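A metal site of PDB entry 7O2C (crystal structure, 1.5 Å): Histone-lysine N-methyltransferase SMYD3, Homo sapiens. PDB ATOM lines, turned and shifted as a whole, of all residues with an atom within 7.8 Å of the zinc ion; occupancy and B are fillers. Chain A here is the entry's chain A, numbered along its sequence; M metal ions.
The side-chain sulfur (SG) of Cys 62 sits close to the backbone NH (N) of Gln 64 (3.6 Å).
The backbone NH of Cys 62 lies within hydrogen-bond range of the backbone carbonyl oxygen of Ala 68 (2.9 Å).
OE2 of Glu 86 lies within hydrogen-bond range of ND1 of His 83.
The backbone NH (N) of Ala 68 sits close to the side-chain sulfur (SG) of Cys 65 (3.7 Å).
The side-chain sulfur of Cys 65 lies close to the backbone NH of Val 67.
Within 4 Å of the zinc ion: Cys 62, Cys 65, His 83 and Cys 87.
The nearest printed residue that does not touch the zinc ion is Gln 64 (4.5 Å).
The zinc ion is bound by NE2 of His 83, SG of Cys 62, SG of Cys 87 and SG of Cys 65.
The zinc ion has four donor atoms within binding distance.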
ATOM      1  N   ARG A  61      13.348  20.928   0.893  1.00  0.00           N
ATOM      2  CA  ARG A  61      13.808  21.583  -0.339  1.00  0.00           C
ATOM      3  C   ARG A  61      13.197  20.948  -1.584  1.00  0.00           C
ATOM      4  O   ARG A  61      12.801  19.797  -1.569  1.00  0.00           O
ATOM      5  CB  ARG A  61      15.324  21.498  -0.478  1.00  0.00           C
ATOM      6  CG  ARG A  61      15.837  20.070  -0.479  1.00  0.00           C
ATOM      7  CD  ARG A  61      17.276  20.045  -0.070  1.00  0.00           C
ATOM      8  NE  ARG A  61      17.670  18.645  -0.003  1.00  0.00           N
ATOM      9  CZ  ARG A  61      18.937  18.219  -0.042  1.00  0.00           C
ATOM     10  NH1 ARG A  61      19.911  19.073  -0.163  1.00  0.00           N
ATOM     11  NH2 ARG A  61      19.214  16.921   0.006  1.00  0.00           N
ATOM     12  N   CYS A  62      13.240  21.715  -2.659  1.00  0.00           N
ATOM     13  CA  CYS A  62      12.917  21.247  -4.036  1.00  0.00           C
ATOM     14  C   CYS A  62      14.025  20.299  -4.403  1.00  0.00           C
ATOM     15  O   CYS A  62      15.206  20.664  -4.256  1.00  0.00           O
ATOM     16  CB  CYS A  62      12.935  22.386  -5.054  1.00  0.00           C
ATOM     17  SG  CYS A  62      12.671  21.925  -6.797  1.00  0.00           S
ATOM     18  N   SER A  63      13.653  19.105  -4.838  1.00  0.00           N
ATOM     19  CA  SER A  63      14.651  18.083  -5.145  1.00  0.00           C
ATOM     20  C   SER A  63      15.491  18.463  -6.378  1.00  0.00           C
ATOM     21  O   SER A  63      16.678  18.182  -6.353  1.00  0.00           O
ATOM     22  CB  SER A  63      13.990  16.753  -5.271  1.00  0.00           C
ATOM     23  OG  SER A  63      14.893  15.860  -5.769  1.00  0.00           O
ATOM     24  N   GLN A  64      14.882  19.116  -7.387  1.00  0.00           N
ATOM     25  CA  GLN A  64      15.536  19.465  -8.685  1.00  0.00           C
ATOM     26  C   GLN A  64      16.609  20.498  -8.390  1.00  0.00           C
ATOM     27  O   GLN A  64      17.746  20.229  -8.734  1.00  0.00           O
ATOM     28  CB  GLN A  64      14.513  19.899  -9.745  1.00  0.00           C
ATOM     29  CG  GLN A  64      13.630  18.754 -10.255  1.00  0.00           C
ATOM     30  CD  GLN A  64      12.304  18.568  -9.539  1.00  0.00           C
ATOM     31  OE1 GLN A  64      11.232  18.768 -10.116  1.00  0.00           O
ATOM     32  NE2 GLN A  64      12.336  18.126  -8.286  1.00  0.00           N
ATOM     33  N   CYS A  65      16.294  21.608  -7.703  1.00  0.00           N
ATOM     34  CA  CYS A  65      17.290  22.721  -7.597  1.00  0.00           C
ATOM     35  C   CYS A  65      17.950  22.743  -6.215  1.00  0.00           C
ATOM     36  O   CYS A  65      19.060  23.225  -6.099  1.00  0.00           O
ATOM     37  CB  CYS A  65      16.628  24.063  -7.922  1.00  0.00           C
ATOM     38  SG  CYS A  65      15.362  24.530  -6.737  1.00  0.00           S
ATOM     39  N   ARG A  66      17.306  22.153  -5.226  1.00  0.00           N
ATOM     40  CA  ARG A  66      17.647  22.273  -3.790  1.00  0.00           C
ATOM     41  C   ARG A  66      17.897  23.714  -3.362  1.00  0.00           C
ATOM     42  O   ARG A  66      18.607  23.879  -2.348  1.00  0.00           O
ATOM     43  CB  ARG A  66      18.855  21.400  -3.486  1.00  0.00           C
ATOM     44  CG  ARG A  66      18.499  19.932  -3.695  1.00  0.00           C
ATOM     45  CD  ARG A  66      19.701  19.064  -3.458  1.00  0.00           C
ATOM     46  NE  ARG A  66      19.324  17.671  -3.427  1.00  0.00           N
ATOM     47  CZ  ARG A  66      20.188  16.672  -3.219  1.00  0.00           C
ATOM     48  NH1 ARG A  66      21.475  16.950  -2.952  1.00  0.00           N
ATOM     49  NH2 ARG A  66      19.747  15.402  -3.237  1.00  0.00           N
ATOM     50  N   VAL A  67      17.297  24.715  -4.009  1.00  0.00           N
ATOM     51  CA  VAL A  67      17.438  26.105  -3.480  1.00  0.00           C
ATOM     52  C   VAL A  67      16.129  26.523  -2.793  1.00  0.00           C
ATOM     53  O   VAL A  67      16.158  27.096  -1.673  1.00  0.00           O
ATOM     54  CB  VAL A  67      17.799  27.071  -4.612  1.00  0.00           C
ATOM     55  CG1 VAL A  67      17.765  28.500  -4.120  1.00  0.00           C
ATOM     56  CG2 VAL A  67      19.143  26.717  -5.221  1.00  0.00           C
ATOM     57  N   ALA A  68      15.016  26.307  -3.488  1.00  0.00           N
ATOM     58  CA  ALA A  68      13.675  26.622  -2.979  1.00  0.00           C
ATOM     59  C   ALA A  68      13.395  25.695  -1.795  1.00  0.00           C
ATOM     60  O   ALA A  68      13.678  24.509  -1.941  1.00  0.00           O
ATOM     61  CB  ALA A  68      12.668  26.460  -4.097  1.00  0.00           C
ATOM     62  N   LYS A  69      12.821  26.208  -0.696  1.00  0.00           N
ATOM     63  CA  LYS A  69      12.454  25.365   0.484  1.00  0.00           C
ATOM     64  C   LYS A  69      11.063  25.752   0.955  1.00  0.00           C
ATOM     65  O   LYS A  69      10.633  26.906   0.773  1.00  0.00           O
ATOM     66  CB  LYS A  69      13.496  25.429   1.604  1.00  0.00           C
ATOM     67  CG  LYS A  69      14.879  25.113   1.099  1.00  0.00           C
ATOM     68  CD  LYS A  69      15.954  24.871   2.118  1.00  0.00           C
ATOM     69  CE  LYS A  69      17.271  24.656   1.389  1.00  0.00           C
ATOM     70  NZ  LYS A  69      18.454  25.177   2.121  1.00  0.00           N
ATOM     71  N   TYR A  70      10.340  24.780   1.469  1.00  0.00           N
ATOM     72  CA  TYR A  70       8.894  24.958   1.696  1.00  0.00           C
ATOM     73  C   TYR A  70       8.564  24.376   3.065  1.00  0.00           C
ATOM     74  O   TYR A  70       9.260  23.463   3.575  1.00  0.00           O
ATOM     75  CB  TYR A  70       8.125  24.246   0.604  1.00  0.00           C
ATOM     76  CG  TYR A  70       8.488  24.739  -0.760  1.00  0.00           C
ATOM     77  CD1 TYR A  70       7.925  25.910  -1.239  1.00  0.00           C
ATOM     78  CD2 TYR A  70       9.356  24.023  -1.590  1.00  0.00           C
ATOM     79  CE1 TYR A  70       8.239  26.372  -2.519  1.00  0.00           C
ATOM     80  CE2 TYR A  70       9.690  24.483  -2.841  1.00  0.00           C
ATOM     81  CZ  TYR A  70       9.114  25.637  -3.308  1.00  0.00           C
ATOM     82  OH  TYR A  70       9.388  26.100  -4.547  1.00  0.00           O
ATOM     83  N   GLN A  76       4.931  23.514  -1.381  1.00  0.00           N
ATOM     84  CA  GLN A  76       5.907  23.137  -2.449  1.00  0.00           C
ATOM     85  C   GLN A  76       5.134  22.919  -3.747  1.00  0.00           C
ATOM     86  O   GLN A  76       5.584  23.376  -4.826  1.00  0.00           O
ATOM     87  CB  GLN A  76       6.664  21.847  -2.108  1.00  0.00           C
ATOM     88  CG  GLN A  76       7.650  21.444  -3.193  1.00  0.00           C
ATOM     89  CD  GLN A  76       8.689  20.420  -2.787  1.00  0.00           C
ATOM     90  OE1 GLN A  76       8.820  20.067  -1.625  1.00  0.00           O
ATOM     91  NE2 GLN A  76       9.452  19.926  -3.769  1.00  0.00           N
ATOM     92  N   TRP A  80       4.833  25.407  -7.441  1.00  0.00           N
ATOM     93  CA  TRP A  80       5.557  24.787  -8.600  1.00  0.00           C
ATOM     94  C   TRP A  80       5.363  25.644  -9.851  1.00  0.00           C
ATOM     95  O   TRP A  80       6.363  25.839 -10.546  1.00  0.00           O
ATOM     96  CB  TRP A  80       5.215  23.314  -8.816  1.00  0.00           C
ATOM     97  CG  TRP A  80       5.838  22.726 -10.033  1.00  0.00           C
ATOM     98  CD1 TRP A  80       5.169  22.337 -11.174  1.00  0.00           C
ATOM     99  CD2 TRP A  80       7.243  22.523 -10.283  1.00  0.00           C
ATOM    100  NE1 TRP A  80       6.059  21.919 -12.119  1.00  0.00           N
ATOM    101  CE2 TRP A  80       7.330  21.983 -11.596  1.00  0.00           C
ATOM    102  CE3 TRP A  80       8.404  22.678  -9.547  1.00  0.00           C
ATOM    103  CZ2 TRP A  80       8.561  21.658 -12.180  1.00  0.00           C
ATOM    104  CZ3 TRP A  80       9.611  22.357 -10.127  1.00  0.00           C
ATOM    105  CH2 TRP A  80       9.693  21.874 -11.422  1.00  0.00           C
ATOM    106  N   HIS A  83       7.593  28.458  -9.862  1.00  0.00           N
ATOM    107  CA  HIS A  83       8.999  28.043  -9.627  1.00  0.00           C
ATOM    108  C   HIS A  83       9.598  27.252 -10.819  1.00  0.00           C
ATOM    109  O   HIS A  83      10.840  27.156 -10.892  1.00  0.00           O
ATOM    110  CB  HIS A  83       9.012  27.229  -8.347  1.00  0.00           C
ATOM    111  CG  HIS A  83      10.340  26.660  -8.079  1.00  0.00           C
ATOM    112  ND1 HIS A  83      11.438  27.441  -7.857  1.00  0.00           N
ATOM    113  CD2 HIS A  83      10.757  25.379  -8.087  1.00  0.00           C
ATOM    114  CE1 HIS A  83      12.483  26.662  -7.669  1.00  0.00           C
ATOM    115  NE2 HIS A  83      12.100  25.411  -7.838  1.00  0.00           N
ATOM    116  N   LYS A  84       8.766  26.650 -11.687  1.00  0.00           N
ATOM    117  CA  LYS A  84       9.152  25.647 -12.702  1.00  0.00           C
ATOM    118  C   LYS A  84      10.333  26.152 -13.531  1.00  0.00           C
ATOM    119  O   LYS A  84      11.367  25.423 -13.607  1.00  0.00           O
ATOM    120  CB  LYS A  84       7.890  25.342 -13.535  1.00  0.00           C
ATOM    121  CG  LYS A  84       8.049  24.437 -14.753  1.00  0.00           C
ATOM    122  CD  LYS A  84       6.755  23.823 -15.255  1.00  0.00           C
ATOM    123  CE  LYS A  84       5.537  24.735 -15.250  1.00  0.00           C
ATOM    124  NZ  LYS A  84       5.330  25.374 -16.577  1.00  0.00           N
ATOM    125  N   GLU A  86      12.318  29.001 -13.106  1.00  0.00           N
ATOM    126  CA  GLU A  86      13.497  29.460 -12.341  1.00  0.00           C
ATOM    127  C   GLU A  86      14.251  28.244 -11.832  1.00  0.00           C
ATOM    128  O   GLU A  86      15.462  28.342 -11.552  1.00  0.00           O
ATOM    129  CB  GLU A  86      13.129  30.468 -11.240  1.00  0.00           C
ATOM    130  CG  GLU A  86      12.542  29.854 -10.005  1.00  0.00           C
ATOM    131  CD  GLU A  86      12.491  30.700  -8.735  1.00  0.00           C
ATOM    132  OE1 GLU A  86      12.887  31.882  -8.707  1.00  0.00           O
ATOM    133  OE2 GLU A  86      12.002  30.136  -7.738  1.00  0.00           O
ATOM    134  N   CYS A  87      13.554  27.148 -11.605  1.00  0.00           N
ATOM    135  CA  CYS A  87      14.173  25.936 -11.031  1.00  0.00           C
ATOM    136  C   CYS A  87      15.371  25.509 -11.927  1.00  0.00           C
ATOM    137  O   CYS A  87      16.496  25.303 -11.400  1.00  0.00           O
ATOM    138  CB  CYS A  87      13.125  24.835 -10.930  1.00  0.00           C
ATOM    139  SG  CYS A  87      13.682  23.328 -10.119  1.00  0.00           S
ATOM    140  N   LYS A  88      15.116  25.446 -13.247  1.00  0.00           N
ATOM    141  CA  LYS A  88      16.104  25.019 -14.272  1.00  0.00           C
ATOM    142  C   LYS A  88      17.293  25.982 -14.182  1.00  0.00           C
ATOM    143  O   LYS A  88      18.434  25.534 -14.305  1.00  0.00           O
ATOM    144  CB  LYS A  88      15.423  24.991 -15.653  1.00  0.00           C
ATOM    145  CG  LYS A  88      14.814  23.652 -16.041  1.00  0.00           C
ATOM    146  CD  LYS A  88      15.869  22.643 -16.468  1.00  0.00           C
ATOM    147  CE  LYS A  88      15.681  21.258 -15.880  1.00  0.00           C
ATOM    148  NZ  LYS A  88      14.583  20.509 -16.546  1.00  0.00           N
ATOM    149  N   LEU A  90      18.275  28.050 -11.425  1.00  0.00           N
ATOM    150  CA  LEU A  90      18.940  27.969 -10.097  1.00  0.00           C
ATOM    151  C   LEU A  90      19.843  26.724 -10.056  1.00  0.00           C
ATOM    152  O   LEU A  90      20.927  26.776  -9.414  1.00  0.00           O
ATOM    153  CB  LEU A  90      17.835  27.924  -9.035  1.00  0.00           C
ATOM    154  CG  LEU A  90      17.074  29.232  -8.750  1.00  0.00           C
ATOM    155  CD1 LEU A  90      15.844  28.965  -7.861  1.00  0.00           C
ATOM    156  CD2 LEU A  90      17.987  30.269  -8.110  1.00  0.00           C
ATOM    157  N   LYS A  91      19.401  25.627 -10.705  1.00  0.00           N
ATOM    158  CA  LYS A  91      20.146  24.336 -10.768  1.00  0.00           C
ATOM    159  C   LYS A  91      21.364  24.599 -11.652  1.00  0.00           C
ATOM    160  O   LYS A  91      22.491  24.378 -11.151  1.00  0.00           O
ATOM    161  CB  LYS A  91      19.297  23.223 -11.377  1.00  0.00           C
ATOM    162  CG  LYS A  91      19.775  21.794 -11.102  1.00  0.00           C
ATOM    163  CD  LYS A  91      19.219  20.749 -12.085  1.00  0.00           C
ATOM    164  CE  LYS A  91      19.070  19.324 -11.551  1.00  0.00           C
ATOM    165  NZ  LYS A  91      20.107  18.921 -10.565  1.00  0.00           N
ATOM    166  N   ARG A 103      16.527  37.433  -9.042  1.00  0.00           N
ATOM    167  CA  ARG A 103      15.542  36.364  -8.919  1.00  0.00           C
ATOM    168  C   ARG A 103      14.159  36.971  -9.094  1.00  0.00           C
ATOM    169  O   ARG A 103      13.304  36.333  -9.704  1.00  0.00           O
ATOM    170  CB  ARG A 103      15.737  35.647  -7.588  1.00  0.00           C
ATOM    171  CG  ARG A 103      14.904  34.385  -7.474  1.00  0.00           C
ATOM    172  CD  ARG A 103      15.230  33.549  -6.259  1.00  0.00           C
ATOM    173  NE  ARG A 103      14.317  32.402  -6.180  1.00  0.00           N
ATOM    174  CZ  ARG A 103      14.257  31.553  -5.137  1.00  0.00           C
ATOM    175  NH1 ARG A 103      14.965  31.816  -4.047  1.00  0.00           N
ATOM    176  NH2 ARG A 103      13.444  30.508  -5.156  1.00  0.00           N
HETATM  177 ZN    ZN M   1      13.439  23.788  -7.845  1.00  0.00          ZN
